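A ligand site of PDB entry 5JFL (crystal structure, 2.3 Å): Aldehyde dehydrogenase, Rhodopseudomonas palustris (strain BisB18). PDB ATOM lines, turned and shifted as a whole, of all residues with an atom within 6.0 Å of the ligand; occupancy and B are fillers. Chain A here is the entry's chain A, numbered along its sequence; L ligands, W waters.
OE1 of Glu 419 sits at hydrogen-bond distance from O12 of the ligand. The backbone carbonyl oxygen (O) of Gly 297 lies within hydrogen-bond range of a nitrogen (N7) of the ligand (2.7 Å). O14 of the ligand is in hydrogen-bond range of N of Ile 495 (2.8 Å). A nitrogen (N7) of the ligand sits at hydrogen-bond distance from the backbone carbonyl oxygen of Ile 495, at 3.3 Å. A ring nitrogen (NE2) of His 449 sits at hydrogen-bond distance from a nitrogen (N7) of the ligand, at 2.9 Å. The backbone carbonyl oxygen (O) of Thr 195 sits at hydrogen-bond distance from an oxygen (O5) of the ligand (3.0 Å). The backbone NH (N) of Thr 197 sits at hydrogen-bond distance from an oxygen (O8) of the ligand (3.0 Å). The backbone NH (N) of Gly 279 lies within hydrogen-bond range of an oxygen (O1) of the ligand, at 3.1 Å.
N of Gly 299 is in hydrogen-bond range of OE2 of Glu 419, at 3.1 Å. NE2 of His 449 lies close to SG of Cys 330, 3.5 Å away. The backbone NH (N) of Gly 278 lies within hydrogen-bond range of the backbone carbonyl oxygen (O) of Ala 296, at 3.1 Å. OG1 of Thr 198 sits at hydrogen-bond distance from ND2 of Asn 199, at 3.2 Å. O of Asn 199 is in hydrogen-bond range of OG1 of Thr 203, 2.7 Å away. The backbone NH (N) of Thr 277 sits at hydrogen-bond distance from the backbone carbonyl oxygen (O) of Ile 194. The side-chain hydroxyl of Thr 494 is in hydrogen-bond range of the side-chain hydroxyl of Thr 277. The backbone carbonyl oxygen of Ile 259 lies close to the side-chain amide oxygen of Asn 263 (2.9 Å).
An oxygen (O14) of the ligand lies close to the backbone carbonyl oxygen of Phe 493 (3.4 Å). Ile 194 touches the ligand (CG2 to O5, 3.4 Å). CA of Pro 196 touches O8 of the ligand, at 3.4 Å. OG1 of Thr 198 touches C21 of the ligand, 3.5 Å away. Asn 199 touches the ligand. Ser 221 touches the ligand (O to O5, 3.9 Å). His 223 touches the ligand. CD1 of Ile 259 touches N5 of the ligand, at 3.4 Å. Thr 262 touches the ligand (CG2 to N5, 3.6 Å). Asn 263 touches the ligand. CG2 of Thr 277 touches C19 of the ligand, at 3.4 Å. Gly 278 touches the ligand. CG1 of Ile 282 touches O4 of the ligand (3.3 Å). Ala 296 touches the ligand (CB to O14, 3.4 Å). Ala 298 touches the ligand (CB to O12, 3.2 Å). Gly 299 touches the ligand (N to O13, 3.8 Å). Cys 330 touches the ligand. Met 421 touches the ligand (SD to C13, 3.7 Å). CA of Thr 494 touches O14 of the ligand, 3.5 Å away. Hydrophobic or aromatic side chains that line the ligand: Ile 194, Pro 196, His 223, Ile 259, Ile 282, Ala 296, Ala 298, Met 421, His 449 and Ile 495. Of the 37 residues printed, 26 come within 4 Å of the ligand.
Water W1 bridges an oxygen (O2) of the ligand (2.5 Å) and a ring nitrogen (NE2) of His 223 (3.1 Å).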
ATOM      1  N   ILE A 194      16.461   7.031   2.064  1.00  0.00           N
ATOM      2  CA  ILE A 194      16.836   5.664   2.418  1.00  0.00           C
ATOM      3  C   ILE A 194      17.922   5.236   1.429  1.00  0.00           C
ATOM      4  O   ILE A 194      17.665   5.093   0.229  1.00  0.00           O
ATOM      5  CB  ILE A 194      15.630   4.718   2.388  1.00  0.00           C
ATOM      6  CG1 ILE A 194      14.437   5.382   3.094  1.00  0.00           C
ATOM      7  CG2 ILE A 194      15.964   3.400   3.054  1.00  0.00           C
ATOM      8  CD1 ILE A 194      13.147   4.636   2.950  1.00  0.00           C
ATOM      9  N   THR A 195      19.128   5.037   1.946  1.00  0.00           N
ATOM     10  CA  THR A 195      20.310   4.821   1.125  1.00  0.00           C
ATOM     11  C   THR A 195      20.771   3.368   1.171  1.00  0.00           C
ATOM     12  O   THR A 195      20.556   2.681   2.177  1.00  0.00           O
ATOM     13  CB  THR A 195      21.442   5.742   1.605  1.00  0.00           C
ATOM     14  OG1 THR A 195      21.684   5.524   2.992  1.00  0.00           O
ATOM     15  CG2 THR A 195      21.063   7.197   1.394  1.00  0.00           C
ATOM     16  N   PRO A 196      21.404   2.869   0.096  1.00  0.00           N
ATOM     17  CA  PRO A 196      21.766   1.444   0.054  1.00  0.00           C
ATOM     18  C   PRO A 196      23.103   1.134   0.691  1.00  0.00           C
ATOM     19  O   PRO A 196      23.779   2.029   1.232  1.00  0.00           O
ATOM     20  CB  PRO A 196      21.781   1.157  -1.447  1.00  0.00           C
ATOM     21  CG  PRO A 196      22.235   2.446  -2.046  1.00  0.00           C
ATOM     22  CD  PRO A 196      21.657   3.540  -1.190  1.00  0.00           C
ATOM     23  N   THR A 197      23.505  -0.134   0.632  1.00  0.00           N
ATOM     24  CA  THR A 197      24.807  -0.584   1.098  1.00  0.00           C
ATOM     25  C   THR A 197      25.808  -0.738  -0.031  1.00  0.00           C
ATOM     26  O   THR A 197      26.954  -1.134   0.210  1.00  0.00           O
ATOM     27  CB  THR A 197      24.681  -1.916   1.843  1.00  0.00           C
ATOM     28  OG1 THR A 197      25.937  -2.269   2.423  1.00  0.00           O
ATOM     29  CG2 THR A 197      24.249  -3.017   0.887  1.00  0.00           C
ATOM     30  N   THR A 198      25.404  -0.432  -1.267  1.00  0.00           N
ATOM     31  CA  THR A 198      26.293  -0.503  -2.424  1.00  0.00           C
ATOM     32  C   THR A 198      26.910   0.852  -2.775  1.00  0.00           C
ATOM     33  O   THR A 198      27.995   0.891  -3.364  1.00  0.00           O
ATOM     34  CB  THR A 198      25.536  -1.049  -3.633  1.00  0.00           C
ATOM     35  OG1 THR A 198      24.602  -0.058  -4.100  1.00  0.00           O
ATOM     36  CG2 THR A 198      24.770  -2.299  -3.247  1.00  0.00           C
ATOM     37  N   ASN A 199      26.227   1.951  -2.437  1.00  0.00           N
ATOM     38  CA  ASN A 199      26.776   3.294  -2.589  1.00  0.00           C
ATOM     39  C   ASN A 199      26.475   4.090  -1.333  1.00  0.00           C
ATOM     40  O   ASN A 199      25.705   5.060  -1.353  1.00  0.00           O
ATOM     41  CB  ASN A 199      26.192   3.979  -3.833  1.00  0.00           C
ATOM     42  CG  ASN A 199      26.249   3.111  -5.063  1.00  0.00           C
ATOM     43  OD1 ASN A 199      27.322   2.782  -5.559  1.00  0.00           O
ATOM     44  ND2 ASN A 199      25.077   2.723  -5.563  1.00  0.00           N
ATOM     45  N   THR A 203      25.732   7.920  -2.299  1.00  0.00           N
ATOM     46  CA  THR A 203      24.340   8.358  -2.316  1.00  0.00           C
ATOM     47  C   THR A 203      24.093   9.503  -1.346  1.00  0.00           C
ATOM     48  O   THR A 203      23.327  10.432  -1.642  1.00  0.00           O
ATOM     49  CB  THR A 203      23.420   7.183  -1.990  1.00  0.00           C
ATOM     50  OG1 THR A 203      23.722   6.084  -2.857  1.00  0.00           O
ATOM     51  CG2 THR A 203      21.962   7.569  -2.170  1.00  0.00           C
ATOM     52  N   SER A 221      18.332   7.606   6.353  1.00  0.00           N
ATOM     53  CA  SER A 221      18.150   6.283   6.934  1.00  0.00           C
ATOM     54  C   SER A 221      19.123   5.353   6.218  1.00  0.00           C
ATOM     55  O   SER A 221      18.783   4.750   5.198  1.00  0.00           O
ATOM     56  CB  SER A 221      16.713   5.788   6.808  1.00  0.00           C
ATOM     57  OG  SER A 221      16.550   4.521   7.420  1.00  0.00           O
ATOM     58  N   PRO A 222      20.347   5.222   6.731  1.00  0.00           N
ATOM     59  CA  PRO A 222      21.333   4.361   6.065  1.00  0.00           C
ATOM     60  C   PRO A 222      21.035   2.888   6.278  1.00  0.00           C
ATOM     61  O   PRO A 222      20.366   2.479   7.223  1.00  0.00           O
ATOM     62  CB  PRO A 222      22.655   4.760   6.736  1.00  0.00           C
ATOM     63  CG  PRO A 222      22.260   5.293   8.066  1.00  0.00           C
ATOM     64  CD  PRO A 222      20.911   5.938   7.887  1.00  0.00           C
ATOM     65  N   HIS A 223      21.553   2.091   5.346  1.00  0.00           N
ATOM     66  CA  HIS A 223      21.502   0.645   5.505  1.00  0.00           C
ATOM     67  C   HIS A 223      22.358   0.254   6.707  1.00  0.00           C
ATOM     68  O   HIS A 223      23.504   0.694   6.809  1.00  0.00           O
ATOM     69  CB  HIS A 223      22.024  -0.027   4.230  1.00  0.00           C
ATOM     70  CG  HIS A 223      21.707  -1.491   4.145  1.00  0.00           C
ATOM     71  ND1 HIS A 223      22.292  -2.426   4.968  1.00  0.00           N
ATOM     72  CD2 HIS A 223      20.894  -2.175   3.303  1.00  0.00           C
ATOM     73  CE1 HIS A 223      21.837  -3.625   4.660  1.00  0.00           C
ATOM     74  NE2 HIS A 223      20.991  -3.501   3.651  1.00  0.00           N
ATOM     75  N   PRO A 224      21.837  -0.545   7.637  1.00  0.00           N
ATOM     76  CA  PRO A 224      22.606  -0.867   8.853  1.00  0.00           C
ATOM     77  C   PRO A 224      23.946  -1.538   8.594  1.00  0.00           C
ATOM     78  O   PRO A 224      24.804  -1.505   9.483  1.00  0.00           O
ATOM     79  CB  PRO A 224      21.651  -1.782   9.645  1.00  0.00           C
ATOM     80  CG  PRO A 224      20.602  -2.215   8.667  1.00  0.00           C
ATOM     81  CD  PRO A 224      20.466  -1.100   7.679  1.00  0.00           C
ATOM     82  N   SER A 258      18.109   1.144  11.573  1.00  0.00           N
ATOM     83  CA  SER A 258      17.414  -0.135  11.624  1.00  0.00           C
ATOM     84  C   SER A 258      16.254  -0.119  10.645  1.00  0.00           C
ATOM     85  O   SER A 258      15.920   0.907  10.045  1.00  0.00           O
ATOM     86  CB  SER A 258      16.920  -0.438  13.036  1.00  0.00           C
ATOM     87  OG  SER A 258      16.004   0.547  13.476  1.00  0.00           O
ATOM     88  N   ILE A 259      15.634  -1.297  10.489  1.00  0.00           N
ATOM     89  CA  ILE A 259      14.440  -1.402   9.663  1.00  0.00           C
ATOM     90  C   ILE A 259      13.244  -0.761  10.345  1.00  0.00           C
ATOM     91  O   ILE A 259      12.292  -0.366   9.673  1.00  0.00           O
ATOM     92  CB  ILE A 259      14.180  -2.888   9.318  1.00  0.00           C
ATOM     93  CG1 ILE A 259      13.674  -3.028   7.885  1.00  0.00           C
ATOM     94  CG2 ILE A 259      13.207  -3.520  10.307  1.00  0.00           C
ATOM     95  CD1 ILE A 259      14.764  -2.890   6.846  1.00  0.00           C
ATOM     96  N   THR A 262      13.582   3.129   9.887  1.00  0.00           N
ATOM     97  CA  THR A 262      13.213   3.411   8.492  1.00  0.00           C
ATOM     98  C   THR A 262      11.698   3.464   8.337  1.00  0.00           C
ATOM     99  O   THR A 262      11.166   4.372   7.694  1.00  0.00           O
ATOM    100  CB  THR A 262      13.821   2.348   7.578  1.00  0.00           C
ATOM    101  OG1 THR A 262      15.241   2.310   7.767  1.00  0.00           O
ATOM    102  CG2 THR A 262      13.509   2.662   6.118  1.00  0.00           C
ATOM    103  N   ASN A 263      10.990   2.495   8.908  1.00  0.00           N
ATOM    104  CA  ASN A 263       9.532   2.541   8.927  1.00  0.00           C
ATOM    105  C   ASN A 263       9.034   3.754   9.706  1.00  0.00           C
ATOM    106  O   ASN A 263       8.092   4.426   9.293  1.00  0.00           O
ATOM    107  CB  ASN A 263       8.961   1.250   9.515  1.00  0.00           C
ATOM    108  CG  ASN A 263       9.306   0.034   8.690  1.00  0.00           C
ATOM    109  OD1 ASN A 263      10.104   0.098   7.761  1.00  0.00           O
ATOM    110  ND2 ASN A 263       8.706  -1.097   9.038  1.00  0.00           N
ATOM    111  N   MET A 266       9.172   6.748   7.593  1.00  0.00           N
ATOM    112  CA  MET A 266       8.159   6.762   6.556  1.00  0.00           C
ATOM    113  C   MET A 266       6.774   7.125   7.087  1.00  0.00           C
ATOM    114  O   MET A 266       5.900   7.492   6.292  1.00  0.00           O
ATOM    115  CB  MET A 266       8.100   5.387   5.869  1.00  0.00           C
ATOM    116  CG  MET A 266       9.316   5.067   5.012  1.00  0.00           C
ATOM    117  SD  MET A 266       9.088   3.594   4.004  1.00  0.00           S
ATOM    118  CE  MET A 266       9.473   2.297   5.177  1.00  0.00           C
ATOM    119  N   THR A 277      16.375   4.470  -2.418  1.00  0.00           N
ATOM    120  CA  THR A 277      17.422   4.017  -3.327  1.00  0.00           C
ATOM    121  C   THR A 277      17.820   2.609  -2.900  1.00  0.00           C
ATOM    122  O   THR A 277      18.653   2.441  -2.003  1.00  0.00           O
ATOM    123  CB  THR A 277      18.604   4.982  -3.299  1.00  0.00           C
ATOM    124  OG1 THR A 277      18.184   6.285  -3.720  1.00  0.00           O
ATOM    125  CG2 THR A 277      19.696   4.502  -4.240  1.00  0.00           C
ATOM    126  N   GLY A 278      17.227   1.601  -3.525  1.00  0.00           N
ATOM    127  CA  GLY A 278      17.495   0.232  -3.162  1.00  0.00           C
ATOM    128  C   GLY A 278      16.795  -0.806  -4.035  1.00  0.00           C
ATOM    129  O   GLY A 278      16.727  -0.642  -5.254  1.00  0.00           O
ATOM    130  N   GLY A 279      16.284  -1.862  -3.407  1.00  0.00           N
ATOM    131  CA  GLY A 279      15.645  -2.935  -4.130  1.00  0.00           C
ATOM    132  C   GLY A 279      14.169  -2.674  -4.394  1.00  0.00           C
ATOM    133  O   GLY A 279      13.672  -1.554  -4.204  1.00  0.00           O
ATOM    134  N   PRO A 280      13.444  -3.697  -4.850  1.00  0.00           N
ATOM    135  CA  PRO A 280      12.012  -3.526  -5.135  1.00  0.00           C
ATOM    136  C   PRO A 280      11.157  -3.467  -3.884  1.00  0.00           C
ATOM    137  O   PRO A 280      10.070  -2.879  -3.889  1.00  0.00           O
ATOM    138  CB  PRO A 280      11.679  -4.749  -5.993  1.00  0.00           C
ATOM    139  CG  PRO A 280      12.654  -5.787  -5.550  1.00  0.00           C
ATOM    140  CD  PRO A 280      13.925  -5.045  -5.218  1.00  0.00           C
ATOM    141  N   ALA A 281      11.634  -4.078  -2.795  1.00  0.00           N
ATOM    142  CA  ALA A 281      10.867  -4.101  -1.554  1.00  0.00           C
ATOM    143  C   ALA A 281      10.799  -2.712  -0.923  1.00  0.00           C
ATOM    144  O   ALA A 281       9.740  -2.290  -0.440  1.00  0.00           O
ATOM    145  CB  ALA A 281      11.465  -5.114  -0.578  1.00  0.00           C
ATOM    146  N   ILE A 282      11.927  -1.990  -0.911  1.00  0.00           N
ATOM    147  CA  ILE A 282      11.928  -0.675  -0.279  1.00  0.00           C
ATOM    148  C   ILE A 282      11.259   0.372  -1.167  1.00  0.00           C
ATOM    149  O   ILE A 282      10.611   1.294  -0.670  1.00  0.00           O
ATOM    150  CB  ILE A 282      13.369  -0.274   0.092  1.00  0.00           C
ATOM    151  CG1 ILE A 282      13.391   1.103   0.774  1.00  0.00           C
ATOM    152  CG2 ILE A 282      14.275  -0.286  -1.142  1.00  0.00           C
ATOM    153  CD1 ILE A 282      12.515   1.183   2.001  1.00  0.00           C
ATOM    154  N   ALA A 285       7.703   0.248  -0.747  1.00  0.00           N
ATOM    155  CA  ALA A 285       7.327   0.586   0.622  1.00  0.00           C
ATOM    156  C   ALA A 285       7.130   2.084   0.791  1.00  0.00           C
ATOM    157  O   ALA A 285       6.170   2.519   1.445  1.00  0.00           O
ATOM    158  CB  ALA A 285       8.376   0.075   1.604  1.00  0.00           C
ATOM    159  N   ALA A 296      13.971   4.708  -6.600  1.00  0.00           N
ATOM    160  CA  ALA A 296      15.105   4.249  -7.395  1.00  0.00           C
ATOM    161  C   ALA A 296      15.223   2.742  -7.204  1.00  0.00           C
ATOM    162  O   ALA A 296      15.714   2.267  -6.185  1.00  0.00           O
ATOM    163  CB  ALA A 296      16.385   4.978  -6.986  1.00  0.00           C
ATOM    164  N   GLY A 297      14.778   1.984  -8.207  1.00  0.00           N
ATOM    165  CA  GLY A 297      14.686   0.544  -8.107  1.00  0.00           C
ATOM    166  C   GLY A 297      15.945  -0.171  -8.572  1.00  0.00           C
ATOM    167  O   GLY A 297      16.988   0.436  -8.828  1.00  0.00           O
ATOM    168  N   ALA A 298      15.828  -1.489  -8.669  1.00  0.00           N
ATOM    169  CA  ALA A 298      16.922  -2.364  -9.061  1.00  0.00           C
ATOM    170  C   ALA A 298      16.975  -2.512 -10.584  1.00  0.00           C
ATOM    171  O   ALA A 298      16.088  -2.061 -11.319  1.00  0.00           O
ATOM    172  CB  ALA A 298      16.780  -3.724  -8.400  1.00  0.00           C
ATOM    173  N   GLY A 299      18.039  -3.148 -11.061  1.00  0.00           N
ATOM    174  CA  GLY A 299      18.253  -3.342 -12.481  1.00  0.00           C
ATOM    175  C   GLY A 299      18.792  -4.723 -12.784  1.00  0.00           C
ATOM    176  O   GLY A 299      18.922  -5.571 -11.895  1.00  0.00           O
ATOM    177  N   LEU A 328      28.942  -3.567  -8.411  1.00  0.00           N
ATOM    178  CA  LEU A 328      27.941  -2.967  -7.527  1.00  0.00           C
ATOM    179  C   LEU A 328      27.057  -1.921  -8.193  1.00  0.00           C
ATOM    180  O   LEU A 328      25.866  -1.844  -7.816  1.00  0.00           O
ATOM    181  CB  LEU A 328      28.636  -2.368  -6.292  1.00  0.00           C
ATOM    182  CG  LEU A 328      29.169  -3.340  -5.232  1.00  0.00           C
ATOM    183  CD1 LEU A 328      29.839  -2.562  -4.107  1.00  0.00           C
ATOM    184  CD2 LEU A 328      28.060  -4.217  -4.693  1.00  0.00           C
ATOM    185  N   CYS A 330      24.247  -0.111 -10.191  1.00  0.00           N
ATOM    186  CA  CYS A 330      23.022  -0.591 -10.800  1.00  0.00           C
ATOM    187  C   CYS A 330      23.072  -0.522 -12.319  1.00  0.00           C
ATOM    188  O   CYS A 330      22.269  -1.174 -12.992  1.00  0.00           O
ATOM    189  CB  CYS A 330      21.820   0.198 -10.284  1.00  0.00           C
ATOM    190  SG  CYS A 330      22.045   1.996 -10.314  1.00  0.00           S
ATOM    191  N   THR A 380      24.883 -12.361  -0.262  1.00  0.00           N
ATOM    192  CA  THR A 380      25.418 -11.046   0.079  1.00  0.00           C
ATOM    193  C   THR A 380      26.889 -11.108   0.481  1.00  0.00           C
ATOM    194  O   THR A 380      27.582 -10.086   0.419  1.00  0.00           O
ATOM    195  CB  THR A 380      24.591 -10.399   1.194  1.00  0.00           C
ATOM    196  OG1 THR A 380      24.225 -11.400   2.162  1.00  0.00           O
ATOM    197  CG2 THR A 380      23.329  -9.771   0.619  1.00  0.00           C
ATOM    198  N   GLU A 419      20.092 -10.436 -10.556  1.00  0.00           N
ATOM    199  CA  GLU A 419      20.995  -9.280 -10.434  1.00  0.00           C
ATOM    200  C   GLU A 419      22.118  -9.690  -9.488  1.00  0.00           C
ATOM    201  O   GLU A 419      22.053  -9.449  -8.283  1.00  0.00           O
ATOM    202  CB  GLU A 419      20.243  -8.059  -9.941  1.00  0.00           C
ATOM    203  CG  GLU A 419      21.121  -6.809  -9.845  1.00  0.00           C
ATOM    204  CD  GLU A 419      20.396  -5.610  -9.265  1.00  0.00           C
ATOM    205  OE1 GLU A 419      19.669  -5.783  -8.260  1.00  0.00           O
ATOM    206  OE2 GLU A 419      20.552  -4.503  -9.812  1.00  0.00           O
ATOM    207  N   MET A 421      25.199  -8.639  -9.123  1.00  0.00           N
ATOM    208  CA  MET A 421      26.056  -7.590  -8.582  1.00  0.00           C
ATOM    209  C   MET A 421      27.449  -8.134  -8.263  1.00  0.00           C
ATOM    210  O   MET A 421      28.024  -7.858  -7.209  1.00  0.00           O
ATOM    211  CB  MET A 421      25.416  -6.925  -7.359  1.00  0.00           C
ATOM    212  CG  MET A 421      23.954  -6.561  -7.563  1.00  0.00           C
ATOM    213  SD  MET A 421      23.238  -5.641  -6.185  1.00  0.00           S
ATOM    214  CE  MET A 421      24.172  -4.126  -6.284  1.00  0.00           C
ATOM    215  N   HIS A 449      15.496   0.130 -16.315  1.00  0.00           N
ATOM    216  CA  HIS A 449      16.590   0.805 -15.629  1.00  0.00           C
ATOM    217  C   HIS A 449      17.728   1.136 -16.592  1.00  0.00           C
ATOM    218  O   HIS A 449      17.805   2.262 -17.098  1.00  0.00           O
ATOM    219  CB  HIS A 449      17.100  -0.057 -14.473  1.00  0.00           C
ATOM    220  CG  HIS A 449      17.959   0.681 -13.498  1.00  0.00           C
ATOM    221  ND1 HIS A 449      19.235   1.093 -13.796  1.00  0.00           N
ATOM    222  CD2 HIS A 449      17.719   1.079 -12.227  1.00  0.00           C
ATOM    223  CE1 HIS A 449      19.753   1.724 -12.753  1.00  0.00           C
ATOM    224  NE2 HIS A 449      18.850   1.727 -11.785  1.00  0.00           N
ATOM    225  N   PHE A 493      23.374   9.211  -8.189  1.00  0.00           N
ATOM    226  CA  PHE A 493      23.386   7.849  -7.663  1.00  0.00           C
ATOM    227  C   PHE A 493      22.006   7.390  -7.212  1.00  0.00           C
ATOM    228  O   PHE A 493      21.885   6.314  -6.628  1.00  0.00           O
ATOM    229  CB  PHE A 493      24.391   7.744  -6.508  1.00  0.00           C
ATOM    230  CG  PHE A 493      25.823   7.761  -6.960  1.00  0.00           C
ATOM    231  CD1 PHE A 493      26.483   8.963  -7.172  1.00  0.00           C
ATOM    232  CD2 PHE A 493      26.504   6.578  -7.184  1.00  0.00           C
ATOM    233  CE1 PHE A 493      27.798   8.984  -7.593  1.00  0.00           C
ATOM    234  CE2 PHE A 493      27.812   6.588  -7.611  1.00  0.00           C
ATOM    235  CZ  PHE A 493      28.459   7.793  -7.811  1.00  0.00           C
ATOM    236  N   THR A 494      20.979   8.197  -7.472  1.00  0.00           N
ATOM    237  CA  THR A 494      19.583   7.818  -7.260  1.00  0.00           C
ATOM    238  C   THR A 494      18.891   7.935  -8.615  1.00  0.00           C
ATOM    239  O   THR A 494      18.549   9.032  -9.056  1.00  0.00           O
ATOM    240  CB  THR A 494      18.918   8.701  -6.211  1.00  0.00           C
ATOM    241  OG1 THR A 494      19.542   8.478  -4.936  1.00  0.00           O
ATOM    242  CG2 THR A 494      17.431   8.406  -6.105  1.00  0.00           C
ATOM    243  N   ILE A 495      18.719   6.801  -9.297  1.00  0.00           N
ATOM    244  CA  ILE A 495      18.160   6.749 -10.643  1.00  0.00           C
ATOM    245  C   ILE A 495      16.733   6.243 -10.542  1.00  0.00           C
ATOM    246  O   ILE A 495      16.503   5.092 -10.159  1.00  0.00           O
ATOM    247  CB  ILE A 495      18.997   5.853 -11.559  1.00  0.00           C
ATOM    248  CG1 ILE A 495      20.465   6.266 -11.518  1.00  0.00           C
ATOM    249  CG2 ILE A 495      18.467   5.906 -12.987  1.00  0.00           C
ATOM    250  CD1 ILE A 495      21.402   5.271 -12.141  1.00  0.00           C
ATOM    251  N   ALA A 496      15.773   7.089 -10.892  1.00  0.00           N
ATOM    252  CA  ALA A 496      14.358   6.794 -10.715  1.00  0.00           C
ATOM    253  C   ALA A 496      13.821   6.117 -11.974  1.00  0.00           C
ATOM    254  O   ALA A 496      13.711   6.751 -13.031  1.00  0.00           O
ATOM    255  CB  ALA A 496      13.581   8.061 -10.404  1.00  0.00           C
HETATM  256  P1  LIG L   1      18.206  -3.025   0.113  1.00  0.00           P
HETATM  257  O1  LIG L   1      16.815  -2.836  -0.464  1.00  0.00           O
HETATM  258  O2  LIG L   1      18.204  -4.217   1.045  1.00  0.00           O
HETATM  259  O3  LIG L   1      18.633  -1.693   0.928  1.00  0.00           O
HETATM  260  C1  LIG L   1      18.215  -0.424   0.444  1.00  0.00           C
HETATM  261  C2  LIG L   1      17.648   0.449   1.617  1.00  0.00           C
HETATM  262  O4  LIG L   1      16.373   0.226   1.756  1.00  0.00           O
HETATM  263  C3  LIG L   1      18.292   0.051   2.947  1.00  0.00           C
HETATM  264  O5  LIG L   1      18.503   1.161   3.705  1.00  0.00           O
HETATM  265  C4  LIG L   1      17.264  -0.870   3.625  1.00  0.00           C
HETATM  266  O6  LIG L   1      17.362  -0.764   5.102  1.00  0.00           O
HETATM  267  C5  LIG L   1      16.119  -0.428   3.219  1.00  0.00           C
HETATM  268  N1  LIG L   1      15.176  -1.489   3.104  1.00  0.00           N
HETATM  269  C6  LIG L   1      15.260  -2.589   2.342  1.00  0.00           C
HETATM  270  N2  LIG L   1      14.141  -3.325   2.547  1.00  0.00           N
HETATM  271  C7  LIG L   1      13.361  -2.662   3.434  1.00  0.00           C
HETATM  272  C8  LIG L   1      12.123  -2.954   3.985  1.00  0.00           C
HETATM  273  N3  LIG L   1      11.346  -4.115   3.702  1.00  0.00           N
HETATM  274  N4  LIG L   1      11.553  -2.100   4.855  1.00  0.00           N
HETATM  275  C9  LIG L   1      12.207  -0.954   5.208  1.00  0.00           C
HETATM  276  N5  LIG L   1      13.427  -0.666   4.673  1.00  0.00           N
HETATM  277  C10 LIG L   1      14.000  -1.519   3.781  1.00  0.00           C
HETATM  278  O7  LIG L   1      19.248  -3.278  -1.087  1.00  0.00           O
HETATM  279  P2  LIG L   1      20.831  -3.004  -1.011  1.00  0.00           P
HETATM  280  O8  LIG L   1      21.139  -1.852  -0.081  1.00  0.00           O
HETATM  281  O9  LIG L   1      21.537  -4.253  -0.522  1.00  0.00           O
HETATM  282  O10 LIG L   1      21.362  -2.644  -2.470  1.00  0.00           O
HETATM  283  C11 LIG L   1      21.098  -3.567  -3.516  1.00  0.00           C
HETATM  284  C12 LIG L   1      19.998  -2.997  -4.411  1.00  0.00           C
HETATM  285  O11 LIG L   1      20.002  -1.679  -4.369  1.00  0.00           O
HETATM  286  C13 LIG L   1      20.280  -3.380  -5.866  1.00  0.00           C
HETATM  287  O12 LIG L   1      19.227  -4.036  -6.384  1.00  0.00           O
HETATM  288  C14 LIG L   1      20.496  -2.031  -6.590  1.00  0.00           C
HETATM  289  O13 LIG L   1      19.980  -2.082  -7.976  1.00  0.00           O
HETATM  290  C15 LIG L   1      19.806  -1.201  -5.894  1.00  0.00           C
HETATM  291  N6  LIG L   1      20.313   0.132  -6.110  1.00  0.00           N
HETATM  292  C16 LIG L   1      19.636   0.983  -6.953  1.00  0.00           C
HETATM  293  C17 LIG L   1      20.121   2.272  -7.183  1.00  0.00           C
HETATM  294  C18 LIG L   1      19.337   3.218  -8.134  1.00  0.00           C
HETATM  295  O14 LIG L   1      19.529   4.418  -8.087  1.00  0.00           O
HETATM  296  N7  LIG L   1      18.388   2.675  -9.072  1.00  0.00           N
HETATM  297  C19 LIG L   1      21.278   2.685  -6.571  1.00  0.00           C
HETATM  298  C20 LIG L   1      21.955   1.834  -5.728  1.00  0.00           C
HETATM  299  C21 LIG L   1      21.470   0.545  -5.498  1.00  0.00           C
HETATM  300  O   HOH W   1      19.961  -5.815   1.819  1.00  0.00           O
